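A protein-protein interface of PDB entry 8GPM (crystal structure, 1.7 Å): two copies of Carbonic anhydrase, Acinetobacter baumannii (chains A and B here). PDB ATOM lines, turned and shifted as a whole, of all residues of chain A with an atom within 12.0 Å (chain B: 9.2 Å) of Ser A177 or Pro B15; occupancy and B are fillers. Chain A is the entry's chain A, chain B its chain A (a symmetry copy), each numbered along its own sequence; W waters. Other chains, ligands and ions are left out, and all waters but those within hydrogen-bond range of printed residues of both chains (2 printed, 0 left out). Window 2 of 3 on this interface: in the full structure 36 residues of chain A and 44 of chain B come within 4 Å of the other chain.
N of Leu A176 sits at hydrogen-bond distance from O of Pro B11 (2.9 Å).
O of Leu A176 lies within hydrogen-bond range of N of Val B13 (2.9 Å).
The guanidinium group (NH2) of Arg A183 sits at hydrogen-bond distance from the backbone carbonyl oxygen (O) of Ile B10, 2.8 Å away.
OG of Ser A180 is in hydrogen-bond range of N of Arg A183.
The backbone NH (N) of Val B12 lies within hydrogen-bond range of the backbone carbonyl oxygen (O) of Val B29, 2.8 Å away.
N of Ile B31 is in hydrogen-bond range of O of Val B12.
Among the printed residues, pairs that only touch across the chains: Pro A175 with Pro B11 (3.3 Å), Ser A178 with Val B12 (3.4 Å), Leu A176 with Val B12 (3.4 Å), Arg A183 with Val B12 (3.5 Å), Ser A177 with Val B13 (3.6 Å), Glu A179 with Ile B30 (3.6 Å), Gln A174 with Ile B10 (3.7 Å), Glu A179 with Val B12 (3.7 Å), Pro A175 with Val B13 (3.8 Å), Leu A176 with Ile B10 (3.8 Å), Ser A177 with Pro B15 (3.8 Å) and Val A173 with Ile B10 (3.9 Å).
Of the printed residues of chain B, Val A173 touches Ile B10.
Of chain B, only Val B13 and Pro B15 come within 4 Å of Ser A177.
Of the printed residues of chain B, Ser A178 touches Val B12 (3.4 Å).
Of the printed residues of chain B, Glu A179 touches Val B12 and Ile B30.
Val B12 touches just these residues of chain A: Leu A176, Ser A178, Glu A179 and Arg A183.
Of chain A, only Pro A175, Leu A176 and Ser A177 come within 4 Å of Val B13.
Printed residues of chain A within 4 Å of Ile B30: Glu A179 (3.6 Å).
The nearest printed residue of chain B that does not touch Leu A176 is Ser B14 (5.2 Å).
Printed residues of chain A that touch a printed residue of chain B: Val A173, Gln A174, Pro A175, Leu A176, Ser A177, Ser A178, Glu A179 and Arg A183.
Hydrophobic or aromatic side chains of chain A that line the printed part of chain B: Val A173, Pro A175 and Leu A176.
Of the 21 printed residues of chain B, 6 touch a printed residue of chain A.
Among the printed residues, 15 pairs touch across the chains.
Among the printed residues, no Asp or Glu carboxylate lies within 4 Å of a Lys or Arg side-chain nitrogen of the other chain.
No position is printed for both chains.
Of the 15 pairs that touch across the chains among the printed residues, none has its exchanged pair printed and touching as well.
Water W2 bridges OE2 of Glu B32 (2.7 Å) and OE2 of Glu A179 (2.8 Å).
Water W1 lies within hydrogen-bond range of O of Leu A184, N of Ile B10 and NE of Arg A183.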
ATOM      1  N   VAL A 173       1.055 -18.769 -29.013  1.00  0.00           N
ATOM      2  CA  VAL A 173       1.228 -18.944 -27.577  1.00  0.00           C
ATOM      3  C   VAL A 173       0.585 -17.780 -26.838  1.00  0.00           C
ATOM      4  O   VAL A 173       0.462 -16.668 -27.362  1.00  0.00           O
ATOM      5  CB  VAL A 173       2.715 -19.082 -27.175  1.00  0.00           C
ATOM      6  CG1 VAL A 173       3.352 -20.169 -27.970  1.00  0.00           C
ATOM      7  CG2 VAL A 173       3.469 -17.743 -27.494  1.00  0.00           C
ATOM      8  N   GLN A 174       0.174 -18.057 -25.607  1.00  0.00           N
ATOM      9  CA  GLN A 174      -0.113 -16.984 -24.669  1.00  0.00           C
ATOM     10  C   GLN A 174       1.220 -16.384 -24.218  1.00  0.00           C
ATOM     11  O   GLN A 174       2.124 -17.129 -23.808  1.00  0.00           O
ATOM     12  CB  GLN A 174      -0.896 -17.513 -23.439  1.00  0.00           C
ATOM     13  CG  GLN A 174      -2.416 -17.613 -23.674  1.00  0.00           C
ATOM     14  CD  GLN A 174      -3.077 -16.252 -23.874  1.00  0.00           C
ATOM     15  OE1 GLN A 174      -3.221 -15.472 -22.933  1.00  0.00           O
ATOM     16  NE2 GLN A 174      -3.487 -15.971 -25.108  1.00  0.00           N
ATOM     17  N   PRO A 175       1.383 -15.064 -24.267  1.00  0.00           N
ATOM     18  CA  PRO A 175       2.620 -14.451 -23.759  1.00  0.00           C
ATOM     19  C   PRO A 175       2.792 -14.682 -22.265  1.00  0.00           C
ATOM     20  O   PRO A 175       1.834 -14.954 -21.521  1.00  0.00           O
ATOM     21  CB  PRO A 175       2.429 -12.953 -24.054  1.00  0.00           C
ATOM     22  CG  PRO A 175       0.926 -12.766 -23.984  1.00  0.00           C
ATOM     23  CD  PRO A 175       0.330 -14.073 -24.545  1.00  0.00           C
ATOM     24  N   LEU A 176       4.042 -14.571 -21.819  1.00  0.00           N
ATOM     25  CA  LEU A 176       4.329 -14.536 -20.392  1.00  0.00           C
ATOM     26  C   LEU A 176       3.973 -13.155 -19.880  1.00  0.00           C
ATOM     27  O   LEU A 176       3.999 -12.202 -20.644  1.00  0.00           O
ATOM     28  CB  LEU A 176       5.806 -14.830 -20.120  1.00  0.00           C
ATOM     29  CG  LEU A 176       6.316 -16.167 -20.694  1.00  0.00           C
ATOM     30  CD1 LEU A 176       7.858 -16.235 -20.854  1.00  0.00           C
ATOM     31  CD2 LEU A 176       5.799 -17.310 -19.836  1.00  0.00           C
ATOM     32  N   SER A 177       3.644 -13.023 -18.590  1.00  0.00           N
ATOM     33  CA  SER A 177       3.266 -11.685 -18.118  1.00  0.00           C
ATOM     34  C   SER A 177       4.411 -10.935 -17.452  1.00  0.00           C
ATOM     35  O   SER A 177       4.243  -9.767 -17.079  1.00  0.00           O
ATOM     36  CB  SER A 177       2.061 -11.748 -17.168  1.00  0.00           C
ATOM     37  OG  SER A 177       2.253 -12.666 -16.112  1.00  0.00           O
ATOM     38  N   SER A 178       5.561 -11.577 -17.291  1.00  0.00           N
ATOM     39  CA  SER A 178       6.767 -10.934 -16.803  1.00  0.00           C
ATOM     40  C   SER A 178       7.940 -11.805 -17.225  1.00  0.00           C
ATOM     41  O   SER A 178       7.765 -12.947 -17.660  1.00  0.00           O
ATOM     42  CB  SER A 178       6.746 -10.790 -15.286  1.00  0.00           C
ATOM     43  OG  SER A 178       6.696 -12.090 -14.727  1.00  0.00           O
ATOM     44  N   GLU A 179       9.135 -11.234 -17.141  1.00  0.00           N
ATOM     45  CA  GLU A 179      10.349 -12.009 -17.344  1.00  0.00           C
ATOM     46  C   GLU A 179      10.562 -12.946 -16.158  1.00  0.00           C
ATOM     47  O   GLU A 179       9.971 -12.790 -15.081  1.00  0.00           O
ATOM     48  CB  GLU A 179      11.550 -11.075 -17.493  1.00  0.00           C
ATOM     49  CG  GLU A 179      11.566 -10.332 -18.804  1.00  0.00           C
ATOM     50  CD  GLU A 179      12.806  -9.464 -18.947  1.00  0.00           C
ATOM     51  OE1 GLU A 179      13.883 -10.038 -19.126  1.00  0.00           O
ATOM     52  OE2 GLU A 179      12.696  -8.208 -18.926  1.00  0.00           O
ATOM     53  N   SER A 180      11.440 -13.922 -16.354  1.00  0.00           N
ATOM     54  CA  SER A 180      11.890 -14.766 -15.259  1.00  0.00           C
ATOM     55  C   SER A 180      13.313 -15.202 -15.557  1.00  0.00           C
ATOM     56  O   SER A 180      13.768 -15.158 -16.707  1.00  0.00           O
ATOM     57  CB  SER A 180      10.992 -15.991 -15.078  1.00  0.00           C
ATOM     58  OG  SER A 180      11.151 -16.854 -16.199  1.00  0.00           O
ATOM     59  N   ASP A 181      14.001 -15.663 -14.505  1.00  0.00           N
ATOM     60  CA  ASP A 181      15.382 -16.085 -14.688  1.00  0.00           C
ATOM     61  C   ASP A 181      15.499 -17.364 -15.513  1.00  0.00           C
ATOM     62  O   ASP A 181      16.572 -17.642 -16.060  1.00  0.00           O
ATOM     63  CB  ASP A 181      16.027 -16.311 -13.330  1.00  0.00           C
ATOM     64  CG  ASP A 181      16.434 -15.012 -12.646  1.00  0.00           C
ATOM     65  OD1 ASP A 181      16.400 -13.941 -13.316  1.00  0.00           O
ATOM     66  OD2 ASP A 181      16.780 -15.079 -11.430  1.00  0.00           O
ATOM     67  N   ASP A 182      14.447 -18.175 -15.598  1.00  0.00           N
ATOM     68  CA  ASP A 182      14.550 -19.451 -16.300  1.00  0.00           C
ATOM     69  C   ASP A 182      13.910 -19.442 -17.688  1.00  0.00           C
ATOM     70  O   ASP A 182      13.928 -20.476 -18.375  1.00  0.00           O
ATOM     71  CB  ASP A 182      13.959 -20.581 -15.434  1.00  0.00           C
ATOM     72  CG  ASP A 182      12.457 -20.476 -15.239  1.00  0.00           C
ATOM     73  OD1 ASP A 182      11.837 -19.474 -15.646  1.00  0.00           O
ATOM     74  OD2 ASP A 182      11.886 -21.418 -14.647  1.00  0.00           O
ATOM     75  N   ARG A 183      13.377 -18.313 -18.151  1.00  0.00           N
ATOM     76  CA  ARG A 183      12.761 -18.349 -19.469  1.00  0.00           C
ATOM     77  C   ARG A 183      13.832 -18.468 -20.550  1.00  0.00           C
ATOM     78  O   ARG A 183      14.965 -18.009 -20.384  1.00  0.00           O
ATOM     79  CB  ARG A 183      11.870 -17.117 -19.713  1.00  0.00           C
ATOM     80  CG  ARG A 183      12.566 -15.794 -19.892  1.00  0.00           C
ATOM     81  CD  ARG A 183      11.510 -14.712 -20.344  1.00  0.00           C
ATOM     82  NE  ARG A 183      11.121 -14.807 -21.752  1.00  0.00           N
ATOM     83  CZ  ARG A 183      11.654 -14.039 -22.702  1.00  0.00           C
ATOM     84  NH1 ARG A 183      12.589 -13.147 -22.413  1.00  0.00           N
ATOM     85  NH2 ARG A 183      11.211 -14.141 -23.966  1.00  0.00           N
ATOM     86  N   LEU A 184      13.470 -19.128 -21.643  1.00  0.00           N
ATOM     87  CA  LEU A 184      14.286 -19.126 -22.852  1.00  0.00           C
ATOM     88  C   LEU A 184      14.311 -17.723 -23.473  1.00  0.00           C
ATOM     89  O   LEU A 184      13.311 -17.001 -23.443  1.00  0.00           O
ATOM     90  CB  LEU A 184      13.691 -20.134 -23.845  1.00  0.00           C
ATOM     91  CG  LEU A 184      13.662 -21.594 -23.368  1.00  0.00           C
ATOM     92  CD1 LEU A 184      13.233 -22.524 -24.494  1.00  0.00           C
ATOM     93  CD2 LEU A 184      15.018 -21.998 -22.845  1.00  0.00           C
ATOM     94  N   ILE B  10       9.275 -17.311 -25.832  1.00  0.00           N
ATOM     95  CA  ILE B  10       7.894 -16.827 -25.712  1.00  0.00           C
ATOM     96  C   ILE B  10       7.913 -15.323 -25.461  1.00  0.00           C
ATOM     97  O   ILE B  10       8.592 -14.879 -24.534  1.00  0.00           O
ATOM     98  CB  ILE B  10       7.160 -17.542 -24.555  1.00  0.00           C
ATOM     99  CG1 ILE B  10       7.149 -19.051 -24.815  1.00  0.00           C
ATOM    100  CG2 ILE B  10       5.734 -17.000 -24.384  1.00  0.00           C
ATOM    101  CD1 ILE B  10       6.665 -19.867 -23.579  1.00  0.00           C
ATOM    102  N   PRO B  11       7.123 -14.519 -26.181  1.00  0.00           N
ATOM    103  CA  PRO B  11       7.079 -13.084 -25.853  1.00  0.00           C
ATOM    104  C   PRO B  11       6.594 -12.801 -24.442  1.00  0.00           C
ATOM    105  O   PRO B  11       5.819 -13.566 -23.877  1.00  0.00           O
ATOM    106  CB  PRO B  11       6.117 -12.484 -26.901  1.00  0.00           C
ATOM    107  CG  PRO B  11       5.946 -13.558 -27.956  1.00  0.00           C
ATOM    108  CD  PRO B  11       6.626 -14.815 -27.537  1.00  0.00           C
ATOM    109  N   VAL B  12       7.089 -11.684 -23.874  1.00  0.00           N
ATOM    110  CA  VAL B  12       6.697 -11.200 -22.542  1.00  0.00           C
ATOM    111  C   VAL B  12       5.865  -9.938 -22.767  1.00  0.00           C
ATOM    112  O   VAL B  12       6.340  -8.996 -23.409  1.00  0.00           O
ATOM    113  CB  VAL B  12       7.908 -10.883 -21.629  1.00  0.00           C
ATOM    114  CG1 VAL B  12       7.444 -10.311 -20.265  1.00  0.00           C
ATOM    115  CG2 VAL B  12       8.851 -12.115 -21.395  1.00  0.00           C
ATOM    116  N   VAL B  13       4.620  -9.903 -22.258  1.00  0.00           N
ATOM    117  CA  VAL B  13       3.761  -8.735 -22.474  1.00  0.00           C
ATOM    118  C   VAL B  13       3.174  -8.312 -21.134  1.00  0.00           C
ATOM    119  O   VAL B  13       2.472  -9.103 -20.490  1.00  0.00           O
ATOM    120  CB  VAL B  13       2.634  -8.980 -23.496  1.00  0.00           C
ATOM    121  CG1 VAL B  13       1.767  -7.692 -23.664  1.00  0.00           C
ATOM    122  CG2 VAL B  13       3.208  -9.346 -24.867  1.00  0.00           C
ATOM    123  N   SER B  14       3.453  -7.067 -20.725  1.00  0.00           N
ATOM    124  CA  SER B  14       2.862  -6.535 -19.501  1.00  0.00           C
ATOM    125  C   SER B  14       1.340  -6.564 -19.621  1.00  0.00           C
ATOM    126  O   SER B  14       0.802  -6.173 -20.654  1.00  0.00           O
ATOM    127  CB  SER B  14       3.314  -5.084 -19.261  1.00  0.00           C
ATOM    128  OG  SER B  14       2.547  -4.495 -18.190  1.00  0.00           O
ATOM    129  N   PRO B  15       0.615  -6.971 -18.570  1.00  0.00           N
ATOM    130  CA  PRO B  15      -0.852  -6.851 -18.614  1.00  0.00           C
ATOM    131  C   PRO B  15      -1.335  -5.415 -18.735  1.00  0.00           C
ATOM    132  O   PRO B  15      -2.511  -5.191 -19.062  1.00  0.00           O
ATOM    133  CB  PRO B  15      -1.310  -7.481 -17.286  1.00  0.00           C
ATOM    134  CG  PRO B  15      -0.098  -8.127 -16.683  1.00  0.00           C
ATOM    135  CD  PRO B  15       1.122  -7.560 -17.321  1.00  0.00           C
ATOM    136  N   ASP B  16      -0.468  -4.438 -18.496  1.00  0.00           N
ATOM    137  CA  ASP B  16      -0.812  -3.026 -18.616  1.00  0.00           C
ATOM    138  C   ASP B  16      -0.384  -2.417 -19.948  1.00  0.00           C
ATOM    139  O   ASP B  16      -0.442  -1.194 -20.095  1.00  0.00           O
ATOM    140  CB  ASP B  16      -0.195  -2.259 -17.453  1.00  0.00           C
ATOM    141  CG  ASP B  16      -0.799  -2.676 -16.112  1.00  0.00           C
ATOM    142  OD1 ASP B  16      -2.040  -2.697 -16.018  1.00  0.00           O
ATOM    143  OD2 ASP B  16      -0.053  -2.990 -15.161  1.00  0.00           O
ATOM    144  N   ALA B  17       0.032  -3.233 -20.909  1.00  0.00           N
ATOM    145  CA  ALA B  17       0.220  -2.813 -22.302  1.00  0.00           C
ATOM    146  C   ALA B  17      -0.973  -3.244 -23.160  1.00  0.00           C
ATOM    147  O   ALA B  17      -1.642  -4.246 -22.872  1.00  0.00           O
ATOM    148  CB  ALA B  17       1.506  -3.417 -22.856  1.00  0.00           C
ATOM    149  N   PHE B  18      -1.243  -2.490 -24.230  1.00  0.00           N
ATOM    150  CA  PHE B  18      -2.221  -2.923 -25.214  1.00  0.00           C
ATOM    151  C   PHE B  18      -1.521  -3.387 -26.480  1.00  0.00           C
ATOM    152  O   PHE B  18      -0.824  -2.590 -27.111  1.00  0.00           O
ATOM    153  CB  PHE B  18      -3.189  -1.794 -25.572  1.00  0.00           C
ATOM    154  CG  PHE B  18      -4.179  -2.220 -26.607  1.00  0.00           C
ATOM    155  CD1 PHE B  18      -5.219  -3.056 -26.263  1.00  0.00           C
ATOM    156  CD2 PHE B  18      -4.040  -1.811 -27.928  1.00  0.00           C
ATOM    157  CE1 PHE B  18      -6.136  -3.483 -27.233  1.00  0.00           C
ATOM    158  CE2 PHE B  18      -4.956  -2.230 -28.900  1.00  0.00           C
ATOM    159  CZ  PHE B  18      -5.983  -3.070 -28.555  1.00  0.00           C
ATOM    160  N   VAL B  19      -1.775  -4.636 -26.904  1.00  0.00           N
ATOM    161  CA  VAL B  19      -1.278  -5.135 -28.189  1.00  0.00           C
ATOM    162  C   VAL B  19      -2.488  -5.427 -29.048  1.00  0.00           C
ATOM    163  O   VAL B  19      -3.310  -6.280 -28.686  1.00  0.00           O
ATOM    164  CB  VAL B  19      -0.417  -6.403 -28.024  1.00  0.00           C
ATOM    165  CG1 VAL B  19       0.005  -6.964 -29.406  1.00  0.00           C
ATOM    166  CG2 VAL B  19       0.813  -6.105 -27.151  1.00  0.00           C
ATOM    167  N   VAL B  29      10.507 -10.958 -27.641  1.00  0.00           N
ATOM    168  CA  VAL B  29       9.970  -9.597 -27.546  1.00  0.00           C
ATOM    169  C   VAL B  29       9.519  -9.358 -26.116  1.00  0.00           C
ATOM    170  O   VAL B  29       8.785 -10.175 -25.555  1.00  0.00           O
ATOM    171  CB  VAL B  29       8.750  -9.396 -28.463  1.00  0.00           C
ATOM    172  CG1 VAL B  29       8.242  -7.937 -28.273  1.00  0.00           C
ATOM    173  CG2 VAL B  29       9.056  -9.703 -29.883  1.00  0.00           C
ATOM    174  N   ILE B  30       9.932  -8.247 -25.521  1.00  0.00           N
ATOM    175  CA  ILE B  30       9.497  -7.904 -24.172  1.00  0.00           C
ATOM    176  C   ILE B  30       8.803  -6.550 -24.241  1.00  0.00           C
ATOM    177  O   ILE B  30       9.416  -5.566 -24.664  1.00  0.00           O
ATOM    178  CB  ILE B  30      10.662  -7.839 -23.187  1.00  0.00           C
ATOM    179  CG1 ILE B  30      11.387  -9.183 -23.094  1.00  0.00           C
ATOM    180  CG2 ILE B  30      10.151  -7.410 -21.762  1.00  0.00           C
ATOM    181  CD1 ILE B  30      12.825  -9.021 -22.569  1.00  0.00           C
ATOM    182  N   ILE B  31       7.548  -6.496 -23.788  1.00  0.00           N
ATOM    183  CA  ILE B  31       6.746  -5.274 -23.827  1.00  0.00           C
ATOM    184  C   ILE B  31       6.459  -4.849 -22.392  1.00  0.00           C
ATOM    185  O   ILE B  31       5.875  -5.625 -21.620  1.00  0.00           O
ATOM    186  CB  ILE B  31       5.407  -5.486 -24.580  1.00  0.00           C
ATOM    187  CG1 ILE B  31       5.622  -6.037 -26.000  1.00  0.00           C
ATOM    188  CG2 ILE B  31       4.570  -4.193 -24.575  1.00  0.00           C
ATOM    189  CD1 ILE B  31       6.401  -5.139 -26.848  1.00  0.00           C
ATOM    190  N   GLU B  32       6.783  -3.589 -22.056  1.00  0.00           N
ATOM    191  CA  GLU B  32       6.566  -3.077 -20.705  1.00  0.00           C
ATOM    192  C   GLU B  32       5.203  -2.375 -20.584  1.00  0.00           C
ATOM    193  O   GLU B  32       4.459  -2.205 -21.561  1.00  0.00           O
ATOM    194  CB  GLU B  32       7.699  -2.113 -20.315  1.00  0.00           C
ATOM    195  CG  GLU B  32       9.125  -2.690 -20.289  1.00  0.00           C
ATOM    196  CD  GLU B  32       9.304  -3.874 -19.315  1.00  0.00           C
ATOM    197  OE1 GLU B  32       8.511  -4.000 -18.344  1.00  0.00           O
ATOM    198  OE2 GLU B  32      10.308  -4.610 -19.453  1.00  0.00           O
ATOM    199  N   ALA B  33       4.889  -1.897 -19.374  1.00  0.00           N
ATOM    200  CA  ALA B  33       3.554  -1.338 -19.106  1.00  0.00           C
ATOM    201  C   ALA B  33       3.309  -0.050 -19.884  1.00  0.00           C
ATOM    202  O   ALA B  33       4.230   0.728 -20.150  1.00  0.00           O
ATOM    203  CB  ALA B  33       3.375  -1.034 -17.603  1.00  0.00           C
ATOM    204  N   GLY B  34       2.041   0.197 -20.215  1.00  0.00           N
ATOM    205  CA  GLY B  34       1.665   1.455 -20.839  1.00  0.00           C
ATOM    206  C   GLY B  34       1.896   1.529 -22.331  1.00  0.00           C
ATOM    207  O   GLY B  34       1.539   2.542 -22.955  1.00  0.00           O
ATOM    208  N   VAL B  35       2.480   0.491 -22.933  1.00  0.00           N
ATOM    209  CA  VAL B  35       2.828   0.497 -24.355  1.00  0.00           C
ATOM    210  C   VAL B  35       1.575   0.277 -25.202  1.00  0.00           C
ATOM    211  O   VAL B  35       0.648  -0.428 -24.798  1.00  0.00           O
ATOM    212  CB  VAL B  35       3.877  -0.592 -24.644  1.00  0.00           C
ATOM    213  CG1 VAL B  35       3.994  -0.849 -26.154  1.00  0.00           C
ATOM    214  CG2 VAL B  35       5.259  -0.190 -24.058  1.00  0.00           C
ATOM    215  N   ALA B 163      -3.783   3.554 -25.196  1.00  0.00           N
ATOM    216  CA  ALA B 163      -3.633   2.181 -24.741  1.00  0.00           C
ATOM    217  C   ALA B 163      -4.676   1.865 -23.686  1.00  0.00           C
ATOM    218  O   ALA B 163      -5.272   0.778 -23.693  1.00  0.00           O
ATOM    219  CB  ALA B 163      -2.230   1.955 -24.179  1.00  0.00           C
ATOM    220  N   GLN B 164      -4.952   2.823 -22.791  1.00  0.00           N
ATOM    221  CA  GLN B 164      -5.938   2.551 -21.751  1.00  0.00           C
ATOM    222  C   GLN B 164      -7.344   2.457 -22.331  1.00  0.00           C
ATOM    223  O   GLN B 164      -8.134   1.592 -21.912  1.00  0.00           O
ATOM    224  CB  GLN B 164      -5.851   3.624 -20.664  1.00  0.00           C
ATOM    225  CG  GLN B 164      -4.444   3.657 -20.015  1.00  0.00           C
ATOM    226  CD  GLN B 164      -3.959   2.286 -19.537  1.00  0.00           C
ATOM    227  OE1 GLN B 164      -4.622   1.626 -18.718  1.00  0.00           O
ATOM    228  NE2 GLN B 164      -2.816   1.820 -20.096  1.00  0.00           N
ATOM    229  N   LEU B 167      -7.570  -0.963 -23.973  1.00  0.00           N
ATOM    230  CA  LEU B 167      -7.756  -2.034 -23.003  1.00  0.00           C
ATOM    231  C   LEU B 167      -9.152  -1.973 -22.413  1.00  0.00           C
ATOM    232  O   LEU B 167      -9.740  -3.019 -22.104  1.00  0.00           O
ATOM    233  CB  LEU B 167      -6.713  -1.955 -21.884  1.00  0.00           C
ATOM    234  CG  LEU B 167      -5.277  -2.345 -22.250  1.00  0.00           C
ATOM    235  CD1 LEU B 167      -4.355  -1.753 -21.193  1.00  0.00           C
ATOM    236  CD2 LEU B 167      -5.109  -3.860 -22.354  1.00  0.00           C
ATOM    237  N   ASN B 168      -9.709  -0.757 -22.279  1.00  0.00           N
ATOM    238  CA  ASN B 168     -11.017  -0.573 -21.646  1.00  0.00           C
ATOM    239  C   ASN B 168     -12.166  -0.918 -22.588  1.00  0.00           C
ATOM    240  O   ASN B 168     -13.204  -1.429 -22.157  1.00  0.00           O
ATOM    241  CB  ASN B 168     -11.154   0.879 -21.189  1.00  0.00           C
ATOM    242  CG  ASN B 168     -10.558   1.107 -19.833  1.00  0.00           C
ATOM    243  OD1 ASN B 168     -10.388   0.167 -19.058  1.00  0.00           O
ATOM    244  ND2 ASN B 168     -10.200   2.354 -19.542  1.00  0.00           N
HETATM  245  O   HOH W   1      10.659 -17.514 -23.212  1.00  0.00           O
HETATM  246  O   HOH W   2      10.222  -7.001 -18.274  1.00  0.00           O
